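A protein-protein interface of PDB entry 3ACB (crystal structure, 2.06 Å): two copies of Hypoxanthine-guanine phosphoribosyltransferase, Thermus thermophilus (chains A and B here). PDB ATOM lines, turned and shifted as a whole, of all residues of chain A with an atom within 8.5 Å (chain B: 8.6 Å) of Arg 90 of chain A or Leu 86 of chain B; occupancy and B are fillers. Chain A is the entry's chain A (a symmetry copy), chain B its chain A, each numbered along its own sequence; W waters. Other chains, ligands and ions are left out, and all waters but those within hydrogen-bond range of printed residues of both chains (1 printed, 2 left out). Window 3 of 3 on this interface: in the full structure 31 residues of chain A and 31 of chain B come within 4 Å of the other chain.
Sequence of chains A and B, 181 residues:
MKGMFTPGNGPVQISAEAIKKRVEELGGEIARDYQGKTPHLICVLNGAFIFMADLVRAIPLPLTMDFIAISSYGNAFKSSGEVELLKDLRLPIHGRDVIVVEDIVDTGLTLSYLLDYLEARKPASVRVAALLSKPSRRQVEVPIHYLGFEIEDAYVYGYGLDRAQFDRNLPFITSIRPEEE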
ATOM      1  N   HIS A  40      27.155   5.866 -39.035  1.00  0.00           N
ATOM      2  CA  HIS A  40      27.477   5.757 -37.623  1.00  0.00           C
ATOM      3  C   HIS A  40      26.160   6.043 -36.910  1.00  0.00           C
ATOM      4  O   HIS A  40      25.695   7.179 -36.894  1.00  0.00           O
ATOM      5  CB  HIS A  40      28.528   6.801 -37.242  1.00  0.00           C
ATOM      6  CG  HIS A  40      28.870   6.802 -35.786  1.00  0.00           C
ATOM      7  ND1 HIS A  40      29.387   5.697 -35.143  1.00  0.00           N
ATOM      8  CD2 HIS A  40      28.759   7.770 -34.845  1.00  0.00           C
ATOM      9  CE1 HIS A  40      29.583   5.987 -33.869  1.00  0.00           C
ATOM     10  NE2 HIS A  40      29.210   7.237 -33.662  1.00  0.00           N
ATOM     11  N   ILE A  42      23.749   6.494 -33.718  1.00  0.00           N
ATOM     12  CA  ILE A  42      23.791   6.869 -32.310  1.00  0.00           C
ATOM     13  C   ILE A  42      22.437   6.669 -31.652  1.00  0.00           C
ATOM     14  O   ILE A  42      21.470   7.381 -31.954  1.00  0.00           O
ATOM     15  CB  ILE A  42      24.217   8.340 -32.138  1.00  0.00           C
ATOM     16  CG1 ILE A  42      25.581   8.559 -32.800  1.00  0.00           C
ATOM     17  CG2 ILE A  42      24.280   8.691 -30.655  1.00  0.00           C
ATOM     18  CD1 ILE A  42      26.055  10.007 -32.782  1.00  0.00           C
ATOM     19  N   LEU A  45      19.697   6.651 -25.451  1.00  0.00           N
ATOM     20  CA  LEU A  45      19.260   5.849 -24.305  1.00  0.00           C
ATOM     21  C   LEU A  45      18.337   6.654 -23.390  1.00  0.00           C
ATOM     22  O   LEU A  45      18.428   7.878 -23.355  1.00  0.00           O
ATOM     23  CB  LEU A  45      20.473   5.378 -23.497  1.00  0.00           C
ATOM     24  CG  LEU A  45      21.388   4.348 -24.159  1.00  0.00           C
ATOM     25  CD1 LEU A  45      22.601   4.098 -23.271  1.00  0.00           C
ATOM     26  CD2 LEU A  45      20.610   3.054 -24.391  1.00  0.00           C
ATOM     27  N   MET A  65      28.410   2.087 -34.253  1.00  0.00           N
ATOM     28  CA  MET A  65      27.368   2.669 -33.429  1.00  0.00           C
ATOM     29  C   MET A  65      27.885   3.172 -32.099  1.00  0.00           C
ATOM     30  O   MET A  65      29.000   2.866 -31.694  1.00  0.00           O
ATOM     31  CB  MET A  65      26.213   1.669 -33.221  1.00  0.00           C
ATOM     32  CG  MET A  65      26.599   0.198 -33.176  1.00  0.00           C
ATOM     33  SD  MET A  65      25.168  -0.943 -33.079  1.00  0.00           S
ATOM     34  CE  MET A  65      25.103  -1.585 -34.738  1.00  0.00           C
ATOM     35  N   ASP A  66      27.069   3.981 -31.439  1.00  0.00           N
ATOM     36  CA  ASP A  66      27.428   4.522 -30.146  1.00  0.00           C
ATOM     37  C   ASP A  66      26.139   4.790 -29.390  1.00  0.00           C
ATOM     38  O   ASP A  66      25.048   4.762 -29.968  1.00  0.00           O
ATOM     39  CB  ASP A  66      28.229   5.813 -30.295  1.00  0.00           C
ATOM     40  CG  ASP A  66      29.150   6.061 -29.116  1.00  0.00           C
ATOM     41  OD1 ASP A  66      29.014   5.353 -28.096  1.00  0.00           O
ATOM     42  OD2 ASP A  66      30.005   6.966 -29.201  1.00  0.00           O
ATOM     43  N   PHE A  67      26.274   5.048 -28.098  1.00  0.00           N
ATOM     44  CA  PHE A  67      25.130   5.295 -27.248  1.00  0.00           C
ATOM     45  C   PHE A  67      25.317   6.583 -26.478  1.00  0.00           C
ATOM     46  O   PHE A  67      26.408   6.875 -25.985  1.00  0.00           O
ATOM     47  CB  PHE A  67      24.962   4.130 -26.279  1.00  0.00           C
ATOM     48  CG  PHE A  67      24.678   2.826 -26.957  1.00  0.00           C
ATOM     49  CD1 PHE A  67      23.366   2.381 -27.112  1.00  0.00           C
ATOM     50  CD2 PHE A  67      25.717   2.051 -27.463  1.00  0.00           C
ATOM     51  CE1 PHE A  67      23.093   1.180 -27.761  1.00  0.00           C
ATOM     52  CE2 PHE A  67      25.456   0.850 -28.114  1.00  0.00           C
ATOM     53  CZ  PHE A  67      24.138   0.413 -28.265  1.00  0.00           C
ATOM     54  N   ILE A  68      24.248   7.360 -26.387  1.00  0.00           N
ATOM     55  CA  ILE A  68      24.299   8.613 -25.657  1.00  0.00           C
ATOM     56  C   ILE A  68      23.025   8.722 -24.828  1.00  0.00           C
ATOM     57  O   ILE A  68      21.956   8.265 -25.244  1.00  0.00           O
ATOM     58  CB  ILE A  68      24.417   9.821 -26.625  1.00  0.00           C
ATOM     59  CG1 ILE A  68      24.783  11.084 -25.842  1.00  0.00           C
ATOM     60  CG2 ILE A  68      23.104  10.042 -27.359  1.00  0.00           C
ATOM     61  CD1 ILE A  68      25.069  12.295 -26.721  1.00  0.00           C
ATOM     62  N   LEU A  86      23.629  13.268 -20.118  1.00  0.00           N
ATOM     63  CA  LEU A  86      23.800  12.228 -19.106  1.00  0.00           C
ATOM     64  C   LEU A  86      24.952  11.277 -19.429  1.00  0.00           C
ATOM     65  O   LEU A  86      25.784  10.988 -18.570  1.00  0.00           O
ATOM     66  CB  LEU A  86      22.497  11.442 -18.943  1.00  0.00           C
ATOM     67  CG  LEU A  86      21.270  12.273 -18.552  1.00  0.00           C
ATOM     68  CD1 LEU A  86      20.053  11.368 -18.431  1.00  0.00           C
ATOM     69  CD2 LEU A  86      21.533  12.995 -17.236  1.00  0.00           C
ATOM     70  N   LYS A  87      24.990  10.779 -20.662  1.00  0.00           N
ATOM     71  CA  LYS A  87      26.064   9.884 -21.092  1.00  0.00           C
ATOM     72  C   LYS A  87      26.685  10.456 -22.360  1.00  0.00           C
ATOM     73  O   LYS A  87      25.970  10.886 -23.262  1.00  0.00           O
ATOM     74  CB  LYS A  87      25.536   8.475 -21.371  1.00  0.00           C
ATOM     75  CG  LYS A  87      26.636   7.511 -21.791  1.00  0.00           C
ATOM     76  CD  LYS A  87      26.095   6.158 -22.210  1.00  0.00           C
ATOM     77  CE  LYS A  87      27.224   5.260 -22.698  1.00  0.00           C
ATOM     78  NZ  LYS A  87      26.720   3.955 -23.204  1.00  0.00           N
ATOM     79  N   ASP A  88      28.012  10.450 -22.434  1.00  0.00           N
ATOM     80  CA  ASP A  88      28.705  11.003 -23.590  1.00  0.00           C
ATOM     81  C   ASP A  88      29.140   9.966 -24.630  1.00  0.00           C
ATOM     82  O   ASP A  88      29.184   8.767 -24.351  1.00  0.00           O
ATOM     83  CB  ASP A  88      29.919  11.811 -23.114  1.00  0.00           C
ATOM     84  CG  ASP A  88      30.553  12.616 -24.224  1.00  0.00           C
ATOM     85  OD1 ASP A  88      29.809  13.303 -24.955  1.00  0.00           O
ATOM     86  OD2 ASP A  88      31.795  12.572 -24.362  1.00  0.00           O
ATOM     87  N   LEU A  89      29.450  10.447 -25.831  1.00  0.00           N
ATOM     88  CA  LEU A  89      29.891   9.593 -26.931  1.00  0.00           C
ATOM     89  C   LEU A  89      31.310   9.106 -26.675  1.00  0.00           C
ATOM     90  O   LEU A  89      32.032   9.685 -25.867  1.00  0.00           O
ATOM     91  CB  LEU A  89      29.864  10.368 -28.250  1.00  0.00           C
ATOM     92  CG  LEU A  89      28.524  10.936 -28.723  1.00  0.00           C
ATOM     93  CD1 LEU A  89      28.748  11.793 -29.963  1.00  0.00           C
ATOM     94  CD2 LEU A  89      27.554   9.797 -29.019  1.00  0.00           C
ATOM     95  N   ARG A  90      31.706   8.044 -27.370  1.00  0.00           N
ATOM     96  CA  ARG A  90      33.044   7.490 -27.218  1.00  0.00           C
ATOM     97  C   ARG A  90      33.750   7.406 -28.569  1.00  0.00           C
ATOM     98  O   ARG A  90      34.975   7.484 -28.642  1.00  0.00           O
ATOM     99  CB  ARG A  90      32.971   6.101 -26.581  1.00  0.00           C
ATOM    100  CG  ARG A  90      32.259   6.093 -25.245  1.00  0.00           C
ATOM    101  CD  ARG A  90      32.186   4.699 -24.641  1.00  0.00           C
ATOM    102  NE  ARG A  90      31.253   4.655 -23.517  1.00  0.00           N
ATOM    103  CZ  ARG A  90      31.367   5.395 -22.417  1.00  0.00           C
ATOM    104  NH1 ARG A  90      32.381   6.240 -22.283  1.00  0.00           N
ATOM    105  NH2 ARG A  90      30.460   5.298 -21.454  1.00  0.00           N
ATOM    106  N   LEU A  91      32.975   7.243 -29.638  1.00  0.00           N
ATOM    107  CA  LEU A  91      33.549   7.157 -30.975  1.00  0.00           C
ATOM    108  C   LEU A  91      33.470   8.509 -31.675  1.00  0.00           C
ATOM    109  O   LEU A  91      32.528   9.277 -31.463  1.00  0.00           O
ATOM    110  CB  LEU A  91      32.833   6.089 -31.806  1.00  0.00           C
ATOM    111  CG  LEU A  91      33.253   4.633 -31.554  1.00  0.00           C
ATOM    112  CD1 LEU A  91      32.944   4.229 -30.126  1.00  0.00           C
ATOM    113  CD2 LEU A  91      32.527   3.719 -32.529  1.00  0.00           C
ATOM    114  N   PRO A  92      34.469   8.823 -32.516  1.00  0.00           N
ATOM    115  CA  PRO A  92      34.507  10.094 -33.247  1.00  0.00           C
ATOM    116  C   PRO A  92      33.363  10.199 -34.249  1.00  0.00           C
ATOM    117  O   PRO A  92      32.922   9.192 -34.802  1.00  0.00           O
ATOM    118  CB  PRO A  92      35.861  10.046 -33.961  1.00  0.00           C
ATOM    119  CG  PRO A  92      36.680   9.106 -33.121  1.00  0.00           C
ATOM    120  CD  PRO A  92      35.680   8.031 -32.783  1.00  0.00           C
ATOM    121  N   ILE A  93      32.877  11.411 -34.485  1.00  0.00           N
ATOM    122  CA  ILE A  93      31.821  11.588 -35.471  1.00  0.00           C
ATOM    123  C   ILE A  93      32.274  12.554 -36.562  1.00  0.00           C
ATOM    124  O   ILE A  93      31.639  12.663 -37.611  1.00  0.00           O
ATOM    125  CB  ILE A  93      30.503  12.093 -34.845  1.00  0.00           C
ATOM    126  CG1 ILE A  93      30.683  13.499 -34.286  1.00  0.00           C
ATOM    127  CG2 ILE A  93      30.040  11.125 -33.748  1.00  0.00           C
ATOM    128  CD1 ILE A  93      29.408  14.069 -33.699  1.00  0.00           C
ATOM    129  N   TYR A 117      24.814  19.655 -30.783  1.00  0.00           N
ATOM    130  CA  TYR A 117      25.959  19.028 -30.133  1.00  0.00           C
ATOM    131  C   TYR A 117      26.778  18.221 -31.141  1.00  0.00           C
ATOM    132  O   TYR A 117      28.008  18.255 -31.124  1.00  0.00           O
ATOM    133  CB  TYR A 117      25.471  18.114 -29.009  1.00  0.00           C
ATOM    134  CG  TYR A 117      26.570  17.440 -28.223  1.00  0.00           C
ATOM    135  CD1 TYR A 117      27.327  18.152 -27.293  1.00  0.00           C
ATOM    136  CD2 TYR A 117      26.844  16.083 -28.399  1.00  0.00           C
ATOM    137  CE1 TYR A 117      28.329  17.527 -26.548  1.00  0.00           C
ATOM    138  CE2 TYR A 117      27.845  15.447 -27.663  1.00  0.00           C
ATOM    139  CZ  TYR A 117      28.579  16.175 -26.739  1.00  0.00           C
ATOM    140  OH  TYR A 117      29.555  15.549 -26.000  1.00  0.00           O
ATOM    141  N   ARG A 121      30.824  18.950 -33.853  1.00  0.00           N
ATOM    142  CA  ARG A 121      31.982  18.116 -34.161  1.00  0.00           C
ATOM    143  C   ARG A 121      32.214  17.935 -35.660  1.00  0.00           C
ATOM    144  O   ARG A 121      33.081  17.165 -36.083  1.00  0.00           O
ATOM    145  CB  ARG A 121      31.843  16.758 -33.473  1.00  0.00           C
ATOM    146  CG  ARG A 121      31.699  16.883 -31.970  1.00  0.00           C
ATOM    147  CD  ARG A 121      32.146  15.621 -31.281  1.00  0.00           C
ATOM    148  NE  ARG A 121      32.074  15.726 -29.828  1.00  0.00           N
ATOM    149  CZ  ARG A 121      32.586  14.820 -29.002  1.00  0.00           C
ATOM    150  NH1 ARG A 121      33.203  13.756 -29.493  1.00  0.00           N
ATOM    151  NH2 ARG A 121      32.479  14.976 -27.688  1.00  0.00           N
ATOM    152  N   LEU B  45      26.687  -2.515 -21.513  1.00  0.00           N
ATOM    153  CA  LEU B  45      26.959  -1.907 -22.818  1.00  0.00           C
ATOM    154  C   LEU B  45      28.429  -2.068 -23.204  1.00  0.00           C
ATOM    155  O   LEU B  45      29.282  -2.181 -22.327  1.00  0.00           O
ATOM    156  CB  LEU B  45      26.613  -0.416 -22.789  1.00  0.00           C
ATOM    157  CG  LEU B  45      25.133  -0.051 -22.673  1.00  0.00           C
ATOM    158  CD1 LEU B  45      24.990   1.459 -22.527  1.00  0.00           C
ATOM    159  CD2 LEU B  45      24.389  -0.548 -23.911  1.00  0.00           C
ATOM    160  N   ASN B  46      28.733  -2.074 -24.502  1.00  0.00           N
ATOM    161  CA  ASN B  46      27.745  -1.943 -25.578  1.00  0.00           C
ATOM    162  C   ASN B  46      27.272  -3.305 -26.090  1.00  0.00           C
ATOM    163  O   ASN B  46      26.137  -3.448 -26.548  1.00  0.00           O
ATOM    164  CB  ASN B  46      28.355  -1.200 -26.775  1.00  0.00           C
ATOM    165  CG  ASN B  46      28.683   0.254 -26.474  1.00  0.00           C
ATOM    166  OD1 ASN B  46      29.326   0.929 -27.285  1.00  0.00           O
ATOM    167  ND2 ASN B  46      28.237   0.745 -25.323  1.00  0.00           N
ATOM    168  N   PHE B  67      21.394   0.600 -17.624  1.00  0.00           N
ATOM    169  CA  PHE B  67      22.519   0.330 -18.494  1.00  0.00           C
ATOM    170  C   PHE B  67      23.806   0.779 -17.840  1.00  0.00           C
ATOM    171  O   PHE B  67      23.866   1.842 -17.220  1.00  0.00           O
ATOM    172  CB  PHE B  67      22.323   1.068 -19.814  1.00  0.00           C
ATOM    173  CG  PHE B  67      21.117   0.616 -20.576  1.00  0.00           C
ATOM    174  CD1 PHE B  67      21.232  -0.348 -21.577  1.00  0.00           C
ATOM    175  CD2 PHE B  67      19.859   1.133 -20.281  1.00  0.00           C
ATOM    176  CE1 PHE B  67      20.110  -0.789 -22.275  1.00  0.00           C
ATOM    177  CE2 PHE B  67      18.732   0.700 -20.971  1.00  0.00           C
ATOM    178  CZ  PHE B  67      18.859  -0.266 -21.972  1.00  0.00           C
ATOM    179  N   ILE B  68      24.836  -0.045 -17.968  1.00  0.00           N
ATOM    180  CA  ILE B  68      26.128   0.286 -17.400  1.00  0.00           C
ATOM    181  C   ILE B  68      27.195  -0.068 -18.430  1.00  0.00           C
ATOM    182  O   ILE B  68      27.055  -1.036 -19.182  1.00  0.00           O
ATOM    183  CB  ILE B  68      26.375  -0.493 -16.080  1.00  0.00           C
ATOM    184  CG1 ILE B  68      27.582   0.095 -15.344  1.00  0.00           C
ATOM    185  CG2 ILE B  68      26.628  -1.963 -16.370  1.00  0.00           C
ATOM    186  CD1 ILE B  68      27.815  -0.503 -13.962  1.00  0.00           C
ATOM    187  N   ALA B  69      28.246   0.739 -18.489  1.00  0.00           N
ATOM    188  CA  ALA B  69      29.331   0.479 -19.426  1.00  0.00           C
ATOM    189  C   ALA B  69      30.608   0.323 -18.622  1.00  0.00           C
ATOM    190  O   ALA B  69      30.961   1.199 -17.835  1.00  0.00           O
ATOM    191  CB  ALA B  69      29.464   1.623 -20.419  1.00  0.00           C
ATOM    192  N   ILE B  70      31.283  -0.805 -18.806  1.00  0.00           N
ATOM    193  CA  ILE B  70      32.525  -1.079 -18.099  1.00  0.00           C
ATOM    194  C   ILE B  70      33.546  -1.687 -19.052  1.00  0.00           C
ATOM    195  O   ILE B  70      33.185  -2.389 -19.997  1.00  0.00           O
ATOM    196  CB  ILE B  70      32.293  -2.049 -16.920  1.00  0.00           C
ATOM    197  CG1 ILE B  70      31.563  -3.301 -17.410  1.00  0.00           C
ATOM    198  CG2 ILE B  70      31.491  -1.362 -15.832  1.00  0.00           C
ATOM    199  CD1 ILE B  70      31.182  -4.261 -16.304  1.00  0.00           C
ATOM    200  N   SER B  71      34.821  -1.409 -18.809  1.00  0.00           N
ATOM    201  CA  SER B  71      35.882  -1.937 -19.658  1.00  0.00           C
ATOM    202  C   SER B  71      37.171  -2.126 -18.868  1.00  0.00           C
ATOM    203  O   SER B  71      37.563  -3.253 -18.570  1.00  0.00           O
ATOM    204  CB  SER B  71      36.127  -0.993 -20.835  1.00  0.00           C
ATOM    205  OG  SER B  71      37.084  -1.533 -21.729  1.00  0.00           O
ATOM    206  N   GLU B  84      37.464  -0.374 -14.552  1.00  0.00           N
ATOM    207  CA  GLU B  84      37.143   0.997 -14.936  1.00  0.00           C
ATOM    208  C   GLU B  84      35.679   1.134 -15.356  1.00  0.00           C
ATOM    209  O   GLU B  84      35.264   0.614 -16.393  1.00  0.00           O
ATOM    210  CB  GLU B  84      38.064   1.450 -16.072  1.00  0.00           C
ATOM    211  CG  GLU B  84      37.807   2.866 -16.564  1.00  0.00           C
ATOM    212  CD  GLU B  84      38.899   3.374 -17.488  1.00  0.00           C
ATOM    213  OE1 GLU B  84      38.685   4.415 -18.144  1.00  0.00           O
ATOM    214  OE2 GLU B  84      39.975   2.742 -17.554  1.00  0.00           O
ATOM    215  N   LEU B  85      34.906   1.842 -14.537  1.00  0.00           N
ATOM    216  CA  LEU B  85      33.487   2.060 -14.793  1.00  0.00           C
ATOM    217  C   LEU B  85      33.283   3.194 -15.794  1.00  0.00           C
ATOM    218  O   LEU B  85      33.446   4.365 -15.454  1.00  0.00           O
ATOM    219  CB  LEU B  85      32.777   2.390 -13.477  1.00  0.00           C
ATOM    220  CG  LEU B  85      31.254   2.535 -13.483  1.00  0.00           C
ATOM    221  CD1 LEU B  85      30.618   1.248 -13.972  1.00  0.00           C
ATOM    222  CD2 LEU B  85      30.770   2.867 -12.078  1.00  0.00           C
ATOM    223  N   LEU B  86      32.921   2.840 -17.025  1.00  0.00           N
ATOM    224  CA  LEU B  86      32.704   3.827 -18.081  1.00  0.00           C
ATOM    225  C   LEU B  86      31.382   4.579 -17.921  1.00  0.00           C
ATOM    226  O   LEU B  86      31.347   5.806 -18.011  1.00  0.00           O
ATOM    227  CB  LEU B  86      32.759   3.144 -19.449  1.00  0.00           C
ATOM    228  CG  LEU B  86      34.064   2.404 -19.764  1.00  0.00           C
ATOM    229  CD1 LEU B  86      33.976   1.772 -21.146  1.00  0.00           C
ATOM    230  CD2 LEU B  86      35.237   3.373 -19.694  1.00  0.00           C
ATOM    231  N   LYS B  87      30.297   3.843 -17.700  1.00  0.00           N
ATOM    232  CA  LYS B  87      28.985   4.457 -17.500  1.00  0.00           C
ATOM    233  C   LYS B  87      28.405   3.935 -16.192  1.00  0.00           C
ATOM    234  O   LYS B  87      28.470   2.739 -15.918  1.00  0.00           O
ATOM    235  CB  LYS B  87      28.033   4.123 -18.650  1.00  0.00           C
ATOM    236  CG  LYS B  87      26.667   4.774 -18.487  1.00  0.00           C
ATOM    237  CD  LYS B  87      25.679   4.326 -19.545  1.00  0.00           C
ATOM    238  CE  LYS B  87      24.309   4.940 -19.291  1.00  0.00           C
ATOM    239  NZ  LYS B  87      23.289   4.451 -20.257  1.00  0.00           N
ATOM    240  N   ASP B  88      27.830   4.827 -15.392  1.00  0.00           N
ATOM    241  CA  ASP B  88      27.275   4.435 -14.102  1.00  0.00           C
ATOM    242  C   ASP B  88      25.762   4.202 -14.105  1.00  0.00           C
ATOM    243  O   ASP B  88      25.055   4.620 -15.024  1.00  0.00           O
ATOM    244  CB  ASP B  88      27.642   5.489 -13.052  1.00  0.00           C
ATOM    245  CG  ASP B  88      27.316   5.045 -11.644  1.00  0.00           C
ATOM    246  OD1 ASP B  88      27.673   3.904 -11.286  1.00  0.00           O
ATOM    247  OD2 ASP B  88      26.710   5.839 -10.891  1.00  0.00           O
ATOM    248  N   LEU B  89      25.280   3.519 -13.069  1.00  0.00           N
ATOM    249  CA  LEU B  89      23.858   3.217 -12.917  1.00  0.00           C
ATOM    250  C   LEU B  89      23.098   4.480 -12.537  1.00  0.00           C
ATOM    251  O   LEU B  89      23.692   5.451 -12.073  1.00  0.00           O
ATOM    252  CB  LEU B  89      23.652   2.167 -11.823  1.00  0.00           C
ATOM    253  CG  LEU B  89      24.312   0.799 -12.007  1.00  0.00           C
ATOM    254  CD1 LEU B  89      24.109  -0.033 -10.747  1.00  0.00           C
ATOM    255  CD2 LEU B  89      23.717   0.095 -13.222  1.00  0.00           C
ATOM    256  N   ARG B  90      21.783   4.459 -12.730  1.00  0.00           N
ATOM    257  CA  ARG B  90      20.946   5.604 -12.396  1.00  0.00           C
ATOM    258  C   ARG B  90      19.820   5.193 -11.452  1.00  0.00           C
ATOM    259  O   ARG B  90      19.345   5.999 -10.655  1.00  0.00           O
ATOM    260  CB  ARG B  90      20.361   6.218 -13.670  1.00  0.00           C
ATOM    261  CG  ARG B  90      21.416   6.629 -14.675  1.00  0.00           C
ATOM    262  CD  ARG B  90      20.807   7.221 -15.937  1.00  0.00           C
ATOM    263  NE  ARG B  90      21.801   7.337 -17.002  1.00  0.00           N
ATOM    264  CZ  ARG B  90      22.920   8.050 -16.911  1.00  0.00           C
ATOM    265  NH1 ARG B  90      23.195   8.722 -15.800  1.00  0.00           N
ATOM    266  NH2 ARG B  90      23.773   8.083 -17.926  1.00  0.00           N
ATOM    267  N   TYR B 113      34.198  -7.933 -11.121  1.00  0.00           N
ATOM    268  CA  TYR B 113      34.254  -6.563 -10.635  1.00  0.00           C
ATOM    269  C   TYR B 113      32.825  -6.057 -10.490  1.00  0.00           C
ATOM    270  O   TYR B 113      32.426  -5.577  -9.428  1.00  0.00           O
ATOM    271  CB  TYR B 113      35.033  -5.682 -11.623  1.00  0.00           C
ATOM    272  CG  TYR B 113      34.902  -4.190 -11.380  1.00  0.00           C
ATOM    273  CD1 TYR B 113      33.711  -3.517 -11.668  1.00  0.00           C
ATOM    274  CD2 TYR B 113      35.963  -3.453 -10.852  1.00  0.00           C
ATOM    275  CE1 TYR B 113      33.580  -2.149 -11.435  1.00  0.00           C
ATOM    276  CE2 TYR B 113      35.841  -2.082 -10.615  1.00  0.00           C
ATOM    277  CZ  TYR B 113      34.645  -1.438 -10.908  1.00  0.00           C
ATOM    278  OH  TYR B 113      34.513  -0.087 -10.677  1.00  0.00           O
ATOM    279  N   GLN B 165      34.608  -2.336 -33.881  1.00  0.00           N
ATOM    280  CA  GLN B 165      33.448  -1.433 -33.913  1.00  0.00           C
ATOM    281  C   GLN B 165      32.421  -1.748 -34.997  1.00  0.00           C
ATOM    282  O   GLN B 165      31.291  -1.256 -34.950  1.00  0.00           O
ATOM    283  CB  GLN B 165      33.891   0.030 -34.054  1.00  0.00           C
ATOM    284  CG  GLN B 165      34.606   0.587 -32.830  1.00  0.00           C
ATOM    285  CD  GLN B 165      33.850   0.314 -31.537  1.00  0.00           C
ATOM    286  OE1 GLN B 165      32.620   0.377 -31.495  1.00  0.00           O
ATOM    287  NE2 GLN B 165      34.588   0.019 -30.474  1.00  0.00           N
ATOM    288  N   ARG B 168      28.290  -5.121 -35.456  1.00  0.00           N
ATOM    289  CA  ARG B 168      27.414  -5.367 -34.315  1.00  0.00           C
ATOM    290  C   ARG B 168      26.004  -5.619 -34.849  1.00  0.00           C
ATOM    291  O   ARG B 168      25.163  -6.201 -34.157  1.00  0.00           O
ATOM    292  CB  ARG B 168      27.339  -4.155 -33.379  1.00  0.00           C
ATOM    293  CG  ARG B 168      28.587  -3.813 -32.585  1.00  0.00           C
ATOM    294  CD  ARG B 168      28.277  -2.620 -31.671  1.00  0.00           C
ATOM    295  NE  ARG B 168      29.468  -2.032 -31.055  1.00  0.00           N
ATOM    296  CZ  ARG B 168      30.138  -2.572 -30.043  1.00  0.00           C
ATOM    297  NH1 ARG B 168      29.738  -3.725 -29.518  1.00  0.00           N
ATOM    298  NH2 ARG B 168      31.213  -1.958 -29.560  1.00  0.00           N
HETATM  299  O   HOH W   1      30.260   0.143 -32.984  1.00  0.00           O
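The side-chain carboxylate (OD2) of Asp 66 of chain A sits at hydrogen-bond distance from the backbone NH (N) of Arg 90 of chain A (2.7 Å).
N of Leu 45 of chain A lies within hydrogen-bond range of O of Ile 68 of chain A, 2.8 Å away.
The backbone NH of Leu 45 of chain B lies within hydrogen-bond range of the backbone carbonyl oxygen of Ile 68 of chain B.
The side-chain amide oxygen (OE1) of Gln 165 of chain B is in hydrogen-bond range of the guanidinium group (NH2) of Arg 168 of chain B (3.3 Å).
The backbone NH (N) of Leu 91 of chain A is in hydrogen-bond range of the side-chain carboxylate (OD2) of Asp 66 of chain A (3.0 Å).
The backbone carbonyl oxygen (O) of Ala 69 of chain B sits at hydrogen-bond distance from the backbone NH (N) of Lys 87 of chain B (2.7 Å).
CD1 of Leu 45 of chain A touches CD1 of Leu 45 of chain B, at 3.6 Å.
Met 65 of chain A touches Arg 168 of chain B (CG to CD, 3.6 Å).
CD2 of Phe 67 of chain A touches ND2 of Asn 46 of chain B, at 3.6 Å.
Leu 45 of chain B touches Lys 87 of chain A (CD1 to NZ, 3.1 Å).
CD of Lys 87 of chain B touches CD of Lys 87 of chain A (3.3 Å).
Lys 87 of chain A touches Arg 90 of chain B (CB to NH2, 3.9 Å).
NH2 of Arg 90 of chain A touches CB of Ala 69 of chain B, 3.9 Å away.
Leu 86 of chain B touches Arg 90 of chain A (O to NH2, 3.6 Å).
Lys 87 of chain B touches Arg 90 of chain A.
Gln 165 of chain B touches Leu 91 of chain A (OE1 to CD2, 3.5 Å).
Of the printed residues of chain B, Leu 45 of chain A touches Leu 45 and Lys 87.
Ile 68 of chain A touches none of the printed residues of chain B.
Of the printed residues of chain B, Leu 86 of chain A touches Arg 90.
Arg 90 of chain A touches three residues of chain B.
Arg 121 of chain A touches none of the printed residues of chain B.
Leu 86 of chain B touches one residue of chain A.
Printed residues of chain A within 4 Å of Lys 87 of chain B: Leu 45, Lys 87 and Arg 90.
The nearest residue of chain B that does not touch Arg 90 of chain A is Asn 46 of chain B (5.3 Å).
The nearest residue of chain A that does not touch Leu 86 of chain B is Lys 87 of chain A (6.3 Å).
The nearest printed residue of chain B that does not touch Phe 67 of chain A is Leu 45 of chain B (4.4 Å).
Of the 17 printed residues of chain A, 7 touch a printed residue of chain B.
Hydrophobic or aromatic side chains of chain A that line the printed part of chain B: Leu 45, Met 65, Phe 67, Leu 86 and Leu 91.
Among the printed residues, no Asp or Glu carboxylate lies within 4 Å of a Lys or Arg side-chain nitrogen of the other chain.
Leu 45 of chain B touches its own counterpart, Leu 45 of chain A.
Leu 86 of chain A touches Arg 90 of chain B, and with the chains exchanged Arg 90 of chain A touches Leu 86 of chain B.
Lys 87 of chain B touches its own counterpart, Lys 87 of chain A.
Lys 87 of chain A touches Arg 90 of chain B, and with the chains exchanged Arg 90 of chain A touches Lys 87 of chain B.
Of the 12 pairs that touch across the chains among the printed residues, 8 have their exchanged pair printed and touching as well.
Water W1 lies within hydrogen-bond range of the backbone carbonyl oxygen of Gln 165 of chain B, the backbone NH of Met 65 of chain A and the guanidinium group of Arg 168 of chain B.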
